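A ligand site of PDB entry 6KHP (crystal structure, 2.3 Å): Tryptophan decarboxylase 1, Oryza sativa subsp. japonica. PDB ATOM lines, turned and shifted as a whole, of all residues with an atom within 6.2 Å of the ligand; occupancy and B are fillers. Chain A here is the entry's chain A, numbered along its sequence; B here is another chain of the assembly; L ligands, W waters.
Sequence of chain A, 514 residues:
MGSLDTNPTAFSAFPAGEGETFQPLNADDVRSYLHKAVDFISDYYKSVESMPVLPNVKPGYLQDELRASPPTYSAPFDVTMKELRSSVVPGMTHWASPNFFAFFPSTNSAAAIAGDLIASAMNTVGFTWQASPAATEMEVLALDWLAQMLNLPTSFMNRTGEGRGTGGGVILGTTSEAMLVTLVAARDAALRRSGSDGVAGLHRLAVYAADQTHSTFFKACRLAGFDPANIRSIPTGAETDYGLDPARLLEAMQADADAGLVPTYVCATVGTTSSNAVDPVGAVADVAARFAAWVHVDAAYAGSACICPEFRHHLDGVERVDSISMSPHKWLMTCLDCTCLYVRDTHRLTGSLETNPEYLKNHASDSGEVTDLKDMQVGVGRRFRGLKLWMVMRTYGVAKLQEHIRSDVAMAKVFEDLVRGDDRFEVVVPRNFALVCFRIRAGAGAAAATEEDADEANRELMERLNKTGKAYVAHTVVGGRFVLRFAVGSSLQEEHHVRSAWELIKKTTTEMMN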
ATOM      1  N   PHE A 104       3.864  21.835 -38.157  1.00  0.00           N
ATOM      2  CA  PHE A 104       4.862  22.815 -37.802  1.00  0.00           C
ATOM      3  C   PHE A 104       6.226  22.152 -37.859  1.00  0.00           C
ATOM      4  O   PHE A 104       6.352  20.987 -37.497  1.00  0.00           O
ATOM      5  CB  PHE A 104       4.633  23.405 -36.407  1.00  0.00           C
ATOM      6  CG  PHE A 104       3.360  24.176 -36.291  1.00  0.00           C
ATOM      7  CD1 PHE A 104       3.172  25.337 -37.010  1.00  0.00           C
ATOM      8  CD2 PHE A 104       2.327  23.723 -35.473  1.00  0.00           C
ATOM      9  CE1 PHE A 104       1.987  26.047 -36.921  1.00  0.00           C
ATOM     10  CE2 PHE A 104       1.132  24.429 -35.371  1.00  0.00           C
ATOM     11  CZ  PHE A 104       0.976  25.593 -36.109  1.00  0.00           C
ATOM     12  N   GLY A 173       6.848  15.322 -22.065  1.00  0.00           N
ATOM     13  CA  GLY A 173       7.052  14.930 -23.439  1.00  0.00           C
ATOM     14  C   GLY A 173       6.132  15.620 -24.424  1.00  0.00           C
ATOM     15  O   GLY A 173       6.534  15.896 -25.554  1.00  0.00           O
ATOM     16  N   THR A 174       4.888  15.937 -24.023  1.00  0.00           N
ATOM     17  CA  THR A 174       3.884  16.393 -24.967  1.00  0.00           C
ATOM     18  C   THR A 174       3.005  17.470 -24.335  1.00  0.00           C
ATOM     19  O   THR A 174       2.872  17.565 -23.120  1.00  0.00           O
ATOM     20  CB  THR A 174       2.969  15.249 -25.452  1.00  0.00           C
ATOM     21  OG1 THR A 174       2.316  14.651 -24.318  1.00  0.00           O
ATOM     22  CG2 THR A 174       3.751  14.172 -26.212  1.00  0.00           C
ATOM     23  N   THR A 175       2.386  18.279 -25.206  1.00  0.00           N
ATOM     24  CA  THR A 175       1.302  19.140 -24.780  1.00  0.00           C
ATOM     25  C   THR A 175       0.128  18.326 -24.239  1.00  0.00           C
ATOM     26  O   THR A 175      -0.535  18.732 -23.284  1.00  0.00           O
ATOM     27  CB  THR A 175       0.860  20.035 -25.939  1.00  0.00           C
ATOM     28  OG1 THR A 175       1.894  20.991 -26.219  1.00  0.00           O
ATOM     29  CG2 THR A 175      -0.442  20.801 -25.629  1.00  0.00           C
ATOM     30  N   SER A 176      -0.124  17.143 -24.810  1.00  0.00           N
ATOM     31  CA  SER A 176      -1.214  16.313 -24.314  1.00  0.00           C
ATOM     32  C   SER A 176      -1.061  15.999 -22.834  1.00  0.00           C
ATOM     33  O   SER A 176      -2.049  16.023 -22.094  1.00  0.00           O
ATOM     34  CB  SER A 176      -1.295  15.001 -25.102  1.00  0.00           C
ATOM     35  OG  SER A 176      -1.622  15.230 -26.451  1.00  0.00           O
ATOM     36  N   GLU A 177       0.151  15.665 -22.384  1.00  0.00           N
ATOM     37  CA  GLU A 177       0.334  15.359 -20.975  1.00  0.00           C
ATOM     38  C   GLU A 177       0.187  16.616 -20.133  1.00  0.00           C
ATOM     39  O   GLU A 177      -0.358  16.561 -19.021  1.00  0.00           O
ATOM     40  CB  GLU A 177       1.705  14.699 -20.731  1.00  0.00           C
ATOM     41  CG  GLU A 177       1.824  14.180 -19.296  1.00  0.00           C
ATOM     42  CD  GLU A 177       3.079  13.389 -19.033  1.00  0.00           C
ATOM     43  OE1 GLU A 177       3.848  13.132 -19.995  1.00  0.00           O
ATOM     44  OE2 GLU A 177       3.319  13.012 -17.859  1.00  0.00           O
ATOM     45  N   MET A 179      -1.801  19.077 -20.879  1.00  0.00           N
ATOM     46  CA  MET A 179      -3.241  19.237 -20.808  1.00  0.00           C
ATOM     47  C   MET A 179      -3.841  18.262 -19.820  1.00  0.00           C
ATOM     48  O   MET A 179      -4.690  18.634 -18.990  1.00  0.00           O
ATOM     49  CB  MET A 179      -3.859  19.047 -22.185  1.00  0.00           C
ATOM     50  CG  MET A 179      -3.606  20.225 -23.091  1.00  0.00           C
ATOM     51  SD  MET A 179      -4.075  19.835 -24.784  1.00  0.00           S
ATOM     52  CE  MET A 179      -4.015  21.453 -25.535  1.00  0.00           C
ATOM     53  N   HIS A 214      -6.572  22.281 -30.533  1.00  0.00           N
ATOM     54  CA  HIS A 214      -6.047  21.027 -31.066  1.00  0.00           C
ATOM     55  C   HIS A 214      -6.859  19.839 -30.552  1.00  0.00           C
ATOM     56  O   HIS A 214      -7.252  19.791 -29.380  1.00  0.00           O
ATOM     57  CB  HIS A 214      -4.580  20.868 -30.687  1.00  0.00           C
ATOM     58  CG  HIS A 214      -3.871  19.793 -31.457  1.00  0.00           C
ATOM     59  ND1 HIS A 214      -4.089  18.448 -31.239  1.00  0.00           N
ATOM     60  CD2 HIS A 214      -2.949  19.862 -32.437  1.00  0.00           C
ATOM     61  CE1 HIS A 214      -3.329  17.738 -32.050  1.00  0.00           C
ATOM     62  NE2 HIS A 214      -2.625  18.578 -32.789  1.00  0.00           N
ATOM     63  N   THR A 216      -6.106  17.055 -29.562  1.00  0.00           N
ATOM     64  CA  THR A 216      -5.604  16.347 -28.396  1.00  0.00           C
ATOM     65  C   THR A 216      -6.145  16.907 -27.078  1.00  0.00           C
ATOM     66  O   THR A 216      -6.168  16.177 -26.085  1.00  0.00           O
ATOM     67  CB  THR A 216      -4.071  16.353 -28.386  1.00  0.00           C
ATOM     68  OG1 THR A 216      -3.610  15.295 -27.536  1.00  0.00           O
ATOM     69  CG2 THR A 216      -3.525  17.701 -27.897  1.00  0.00           C
ATOM     70  N   THR A 269      -5.915  28.867 -26.706  1.00  0.00           N
ATOM     71  CA  THR A 269      -4.782  28.579 -27.575  1.00  0.00           C
ATOM     72  C   THR A 269      -4.226  29.871 -28.150  1.00  0.00           C
ATOM     73  O   THR A 269      -4.983  30.723 -28.649  1.00  0.00           O
ATOM     74  CB  THR A 269      -5.179  27.624 -28.714  1.00  0.00           C
ATOM     75  OG1 THR A 269      -5.709  26.430 -28.155  1.00  0.00           O
ATOM     76  CG2 THR A 269      -3.962  27.271 -29.577  1.00  0.00           C
ATOM     77  N   VAL A 270      -2.913  30.028 -28.054  1.00  0.00           N
ATOM     78  CA  VAL A 270      -2.178  31.099 -28.726  1.00  0.00           C
ATOM     79  C   VAL A 270      -1.384  30.444 -29.847  1.00  0.00           C
ATOM     80  O   VAL A 270      -0.335  29.835 -29.625  1.00  0.00           O
ATOM     81  CB  VAL A 270      -1.265  31.854 -27.747  1.00  0.00           C
ATOM     82  CG1 VAL A 270      -0.475  32.911 -28.487  1.00  0.00           C
ATOM     83  CG2 VAL A 270      -2.092  32.457 -26.639  1.00  0.00           C
ATOM     84  N   GLY A 271      -1.892  30.567 -31.083  1.00  0.00           N
ATOM     85  CA  GLY A 271      -1.258  29.967 -32.251  1.00  0.00           C
ATOM     86  C   GLY A 271      -1.854  28.619 -32.591  1.00  0.00           C
ATOM     87  O   GLY A 271      -1.206  27.586 -32.439  1.00  0.00           O
ATOM     88  N   THR A 272      -3.107  28.620 -33.066  1.00  0.00           N
ATOM     89  CA  THR A 272      -3.805  27.374 -33.302  1.00  0.00           C
ATOM     90  C   THR A 272      -3.095  26.583 -34.411  1.00  0.00           C
ATOM     91  O   THR A 272      -2.398  27.128 -35.257  1.00  0.00           O
ATOM     92  CB  THR A 272      -5.281  27.604 -33.688  1.00  0.00           C
ATOM     93  OG1 THR A 272      -5.380  28.469 -34.832  1.00  0.00           O
ATOM     94  CG2 THR A 272      -6.073  28.210 -32.506  1.00  0.00           C
ATOM     95  N   THR A 273      -3.303  25.265 -34.373  1.00  0.00           N
ATOM     96  CA  THR A 273      -2.633  24.380 -35.316  1.00  0.00           C
ATOM     97  C   THR A 273      -3.085  24.650 -36.764  1.00  0.00           C
ATOM     98  O   THR A 273      -2.256  24.664 -37.676  1.00  0.00           O
ATOM     99  CB  THR A 273      -2.865  22.931 -34.909  1.00  0.00           C
ATOM    100  OG1 THR A 273      -2.376  22.062 -35.936  1.00  0.00           O
ATOM    101  CG2 THR A 273      -4.330  22.634 -34.693  1.00  0.00           C
ATOM    102  N   ASP A 298      -2.542  26.962 -24.121  1.00  0.00           N
ATOM    103  CA  ASP A 298      -1.763  26.118 -25.012  1.00  0.00           C
ATOM    104  C   ASP A 298      -1.073  27.018 -26.037  1.00  0.00           C
ATOM    105  O   ASP A 298      -1.739  27.552 -26.941  1.00  0.00           O
ATOM    106  CB  ASP A 298      -2.637  25.082 -25.725  1.00  0.00           C
ATOM    107  CG  ASP A 298      -1.882  24.294 -26.806  1.00  0.00           C
ATOM    108  OD1 ASP A 298      -0.635  24.382 -26.880  1.00  0.00           O
ATOM    109  OD2 ASP A 298      -2.538  23.578 -27.587  1.00  0.00           O
ATOM    110  N   ALA A 299       0.233  27.184 -25.898  1.00  0.00           N
ATOM    111  CA  ALA A 299       1.041  27.928 -26.865  1.00  0.00           C
ATOM    112  C   ALA A 299       2.118  27.036 -27.457  1.00  0.00           C
ATOM    113  O   ALA A 299       3.273  27.446 -27.614  1.00  0.00           O
ATOM    114  CB  ALA A 299       1.661  29.165 -26.233  1.00  0.00           C
ATOM    115  N   ALA A 300       1.738  25.803 -27.805  1.00  0.00           N
ATOM    116  CA  ALA A 300       2.701  24.780 -28.210  1.00  0.00           C
ATOM    117  C   ALA A 300       3.693  25.294 -29.244  1.00  0.00           C
ATOM    118  O   ALA A 300       4.913  25.181 -29.064  1.00  0.00           O
ATOM    119  CB  ALA A 300       1.969  23.546 -28.749  1.00  0.00           C
ATOM    120  N   TYR A 301       3.182  25.895 -30.316  1.00  0.00           N
ATOM    121  CA  TYR A 301       4.038  26.383 -31.396  1.00  0.00           C
ATOM    122  C   TYR A 301       4.466  27.835 -31.183  1.00  0.00           C
ATOM    123  O   TYR A 301       5.659  28.131 -31.113  1.00  0.00           O
ATOM    124  CB  TYR A 301       3.288  26.233 -32.734  1.00  0.00           C
ATOM    125  CG  TYR A 301       3.877  27.048 -33.856  1.00  0.00           C
ATOM    126  CD1 TYR A 301       5.071  26.672 -34.473  1.00  0.00           C
ATOM    127  CD2 TYR A 301       3.243  28.204 -34.312  1.00  0.00           C
ATOM    128  CE1 TYR A 301       5.616  27.407 -35.512  1.00  0.00           C
ATOM    129  CE2 TYR A 301       3.777  28.958 -35.347  1.00  0.00           C
ATOM    130  CZ  TYR A 301       4.962  28.555 -35.941  1.00  0.00           C
ATOM    131  OH  TYR A 301       5.489  29.313 -36.964  1.00  0.00           O
ATOM    132  N   SER A 327       6.064  24.218 -26.496  1.00  0.00           N
ATOM    133  CA  SER A 327       6.995  23.146 -26.799  1.00  0.00           C
ATOM    134  C   SER A 327       8.216  23.687 -27.503  1.00  0.00           C
ATOM    135  O   SER A 327       8.134  24.037 -28.691  1.00  0.00           O
ATOM    136  CB  SER A 327       6.327  22.073 -27.665  1.00  0.00           C
ATOM    137  OG  SER A 327       5.139  21.639 -27.052  1.00  0.00           O
ATOM    138  N   HIS A 329      10.303  21.852 -28.658  1.00  0.00           N
ATOM    139  CA  HIS A 329      10.519  20.912 -29.753  1.00  0.00           C
ATOM    140  C   HIS A 329       9.697  21.256 -30.990  1.00  0.00           C
ATOM    141  O   HIS A 329       9.728  20.495 -31.968  1.00  0.00           O
ATOM    142  CB  HIS A 329      10.279  19.458 -29.323  1.00  0.00           C
ATOM    143  CG  HIS A 329       8.840  19.076 -29.137  1.00  0.00           C
ATOM    144  ND1 HIS A 329       8.422  18.300 -28.073  1.00  0.00           N
ATOM    145  CD2 HIS A 329       7.734  19.292 -29.889  1.00  0.00           C
ATOM    146  CE1 HIS A 329       7.119  18.094 -28.162  1.00  0.00           C
ATOM    147  NE2 HIS A 329       6.682  18.688 -29.255  1.00  0.00           N
ATOM    148  N   LYS A 330       8.979  22.380 -30.986  1.00  0.00           N
ATOM    149  CA  LYS A 330       8.471  22.911 -32.237  1.00  0.00           C
ATOM    150  C   LYS A 330       9.404  24.006 -32.725  1.00  0.00           C
ATOM    151  O   LYS A 330      10.196  23.788 -33.641  1.00  0.00           O
ATOM    152  CB  LYS A 330       7.033  23.423 -32.068  1.00  0.00           C
ATOM    153  CG  LYS A 330       6.034  22.293 -32.019  1.00  0.00           C
ATOM    154  CD  LYS A 330       4.628  22.744 -32.266  1.00  0.00           C
ATOM    155  CE  LYS A 330       3.852  21.625 -32.967  1.00  0.00           C
ATOM    156  NZ  LYS A 330       2.885  20.980 -32.046  1.00  0.00           N
ATOM    157  N   THR A 339       8.409  19.524 -23.973  1.00  0.00           N
ATOM    158  CA  THR A 339       7.284  20.415 -23.742  1.00  0.00           C
ATOM    159  C   THR A 339       7.391  20.966 -22.339  1.00  0.00           C
ATOM    160  O   THR A 339       7.566  20.207 -21.381  1.00  0.00           O
ATOM    161  CB  THR A 339       5.949  19.709 -23.954  1.00  0.00           C
ATOM    162  OG1 THR A 339       5.797  19.400 -25.330  1.00  0.00           O
ATOM    163  CG2 THR A 339       4.798  20.604 -23.539  1.00  0.00           C
ATOM    164  N   VAL B 378      -0.877   8.727 -24.508  1.00  0.00           N
ATOM    165  CA  VAL B 378      -1.349   9.993 -23.938  1.00  0.00           C
ATOM    166  C   VAL B 378      -1.376  11.079 -25.016  1.00  0.00           C
ATOM    167  O   VAL B 378      -2.436  11.622 -25.349  1.00  0.00           O
ATOM    168  CB  VAL B 378      -0.490  10.399 -22.721  1.00  0.00           C
ATOM    169  CG1 VAL B 378      -0.531  11.907 -22.477  1.00  0.00           C
ATOM    170  CG2 VAL B 378      -0.998   9.680 -21.505  1.00  0.00           C
ATOM    171  N   GLY B 379      -0.229  11.366 -25.609  1.00  0.00           N
ATOM    172  CA  GLY B 379      -0.197  12.267 -26.737  1.00  0.00           C
ATOM    173  C   GLY B 379       0.414  11.614 -27.962  1.00  0.00           C
ATOM    174  O   GLY B 379       1.570  11.186 -27.924  1.00  0.00           O
ATOM    175  N   VAL B 380      -0.359  11.499 -29.043  1.00  0.00           N
ATOM    176  CA  VAL B 380       0.254  11.155 -30.326  1.00  0.00           C
ATOM    177  C   VAL B 380       1.010  12.377 -30.814  1.00  0.00           C
ATOM    178  O   VAL B 380       0.520  13.511 -30.698  1.00  0.00           O
ATOM    179  CB  VAL B 380      -0.782  10.695 -31.359  1.00  0.00           C
ATOM    180  CG1 VAL B 380      -0.103   9.856 -32.439  1.00  0.00           C
ATOM    181  CG2 VAL B 380      -1.937   9.955 -30.697  1.00  0.00           C
ATOM    182  N   GLY B 381       2.204  12.161 -31.335  1.00  0.00           N
ATOM    183  CA  GLY B 381       3.076  13.279 -31.629  1.00  0.00           C
ATOM    184  C   GLY B 381       4.317  13.259 -30.756  1.00  0.00           C
ATOM    185  O   GLY B 381       4.527  14.187 -29.959  1.00  0.00           O
ATOM    186  N   ARG B 382       5.132  12.203 -30.880  1.00  0.00           N
ATOM    187  CA  ARG B 382       6.388  12.112 -30.138  1.00  0.00           C
ATOM    188  C   ARG B 382       7.426  11.407 -31.017  1.00  0.00           C
ATOM    189  O   ARG B 382       7.141  10.985 -32.149  1.00  0.00           O
ATOM    190  CB  ARG B 382       6.171  11.417 -28.786  1.00  0.00           C
ATOM    191  CG  ARG B 382       5.321  10.139 -28.834  1.00  0.00           C
ATOM    192  CD  ARG B 382       6.047   8.987 -29.518  1.00  0.00           C
ATOM    193  NE  ARG B 382       5.243   7.775 -29.577  1.00  0.00           N
ATOM    194  CZ  ARG B 382       5.649   6.619 -30.096  1.00  0.00           C
ATOM    195  NH1 ARG B 382       6.877   6.501 -30.605  1.00  0.00           N
ATOM    196  NH2 ARG B 382       4.829   5.582 -30.097  1.00  0.00           N
HETATM  197  N1  LIG L   1      -1.383  22.142 -29.572  1.00  0.00           N
HETATM  198  C1  LIG L   1      -0.943  23.019 -30.557  1.00  0.00           C
HETATM  199  C2  LIG L   1      -1.475  24.420 -30.654  1.00  0.00           C
HETATM  200  C3  LIG L   1       0.020  22.598 -31.473  1.00  0.00           C
HETATM  201  O1  LIG L   1       0.443  23.476 -32.433  1.00  0.00           O
HETATM  202  C4  LIG L   1       0.543  21.301 -31.404  1.00  0.00           C
HETATM  203  C5  LIG L   1       1.520  20.800 -32.439  1.00  0.00           C
HETATM  204  C6  LIG L   1       0.099  20.415 -30.417  1.00  0.00           C
HETATM  205  C7  LIG L   1      -0.879  20.853 -29.507  1.00  0.00           C
HETATM  206  C8  LIG L   1       0.668  19.012 -30.352  1.00  0.00           C
HETATM  207  O2  LIG L   1       0.399  18.387 -29.110  1.00  0.00           O
HETATM  208  P1  LIG L   1       1.280  17.097 -28.602  1.00  0.00           P
HETATM  209  O3  LIG L   1       2.692  17.549 -28.207  1.00  0.00           O
HETATM  210  O4  LIG L   1       0.588  16.460 -27.405  1.00  0.00           O
HETATM  211  O5  LIG L   1       1.370  16.063 -29.704  1.00  0.00           O
HETATM  212  O   HOH W   1       3.591  19.937 -28.582  1.00  0.00           O
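O of Asp 298 sits at hydrogen-bond distance from N of Val 270 (3.0 Å).
The side-chain hydroxyl (OG) of Ser 327 sits at hydrogen-bond distance from the side-chain hydroxyl (OG1) of Thr 175.
N of Thr 216 sits at hydrogen-bond distance from ND1 of His 214 (3.0 Å).
The backbone NH (N) of Ser 327 lies within hydrogen-bond range of the backbone carbonyl oxygen (O) of Ala 300, 3.0 Å away.
The backbone NH (N) of Ala 300 lies within hydrogen-bond range of the side-chain carboxylate (OD1) of Asp 298.
OG1 of Thr 174 sits at hydrogen-bond distance from N of Glu 177 (3.1 Å).
Water W1 lies within hydrogen-bond range of an oxygen (O3) of the ligand (2.6 Å), the side-chain hydroxyl (OG) of Ser 327 (2.8 Å), the side-chain hydroxyl (OG1) of Thr 175 (3.1 Å) and a ring nitrogen (NE2) of His 329 (3.4 Å).
CE2 of Phe 104 touches O1 of the ligand, at 3.2 Å.
Thr 174 touches the ligand (CB to O4, 3.3 Å).
CB of His 214 touches N1 of the ligand, 3.6 Å away.
Thr 269 touches the ligand.
O of Gly 271 touches C2 of the ligand (3.6 Å).
Ala 300 touches the ligand.
CB of Tyr 301 touches O1 of the ligand, 3.97 Å away.
O of Gly 381 of chain B touches O5 of the ligand, at 3.7 Å.
Within 4 Å of the ligand: Phe 104, Thr 174, Thr 175, Ser 176, His 214, Thr 269, Gly 271, Asp 298, Ala 300, Tyr 301, Lys 330, Val 380 of chain B and Gly 381 of chain B.
The nearest printed residue that does not touch the ligand is Thr 216 (4.2 Å).
N of Ser 176 sits at hydrogen-bond distance from O4 of the ligand.
O of Val 380 of chain B lies close to O5 of the ligand (2.9 Å).
The side-chain hydroxyl (OG) of Ser 176 sits at hydrogen-bond distance from an oxygen (O4) of the ligand (2.7 Å).
OD2 of Asp 298 lies within hydrogen-bond range of N1 of the ligand, 2.7 Å away.
NZ of Lys 330 is bonded to C5 of the ligand.
An oxygen (O3) of the ligand lies within hydrogen-bond range of the backbone NH (N) of Thr 175 (3.1 Å).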
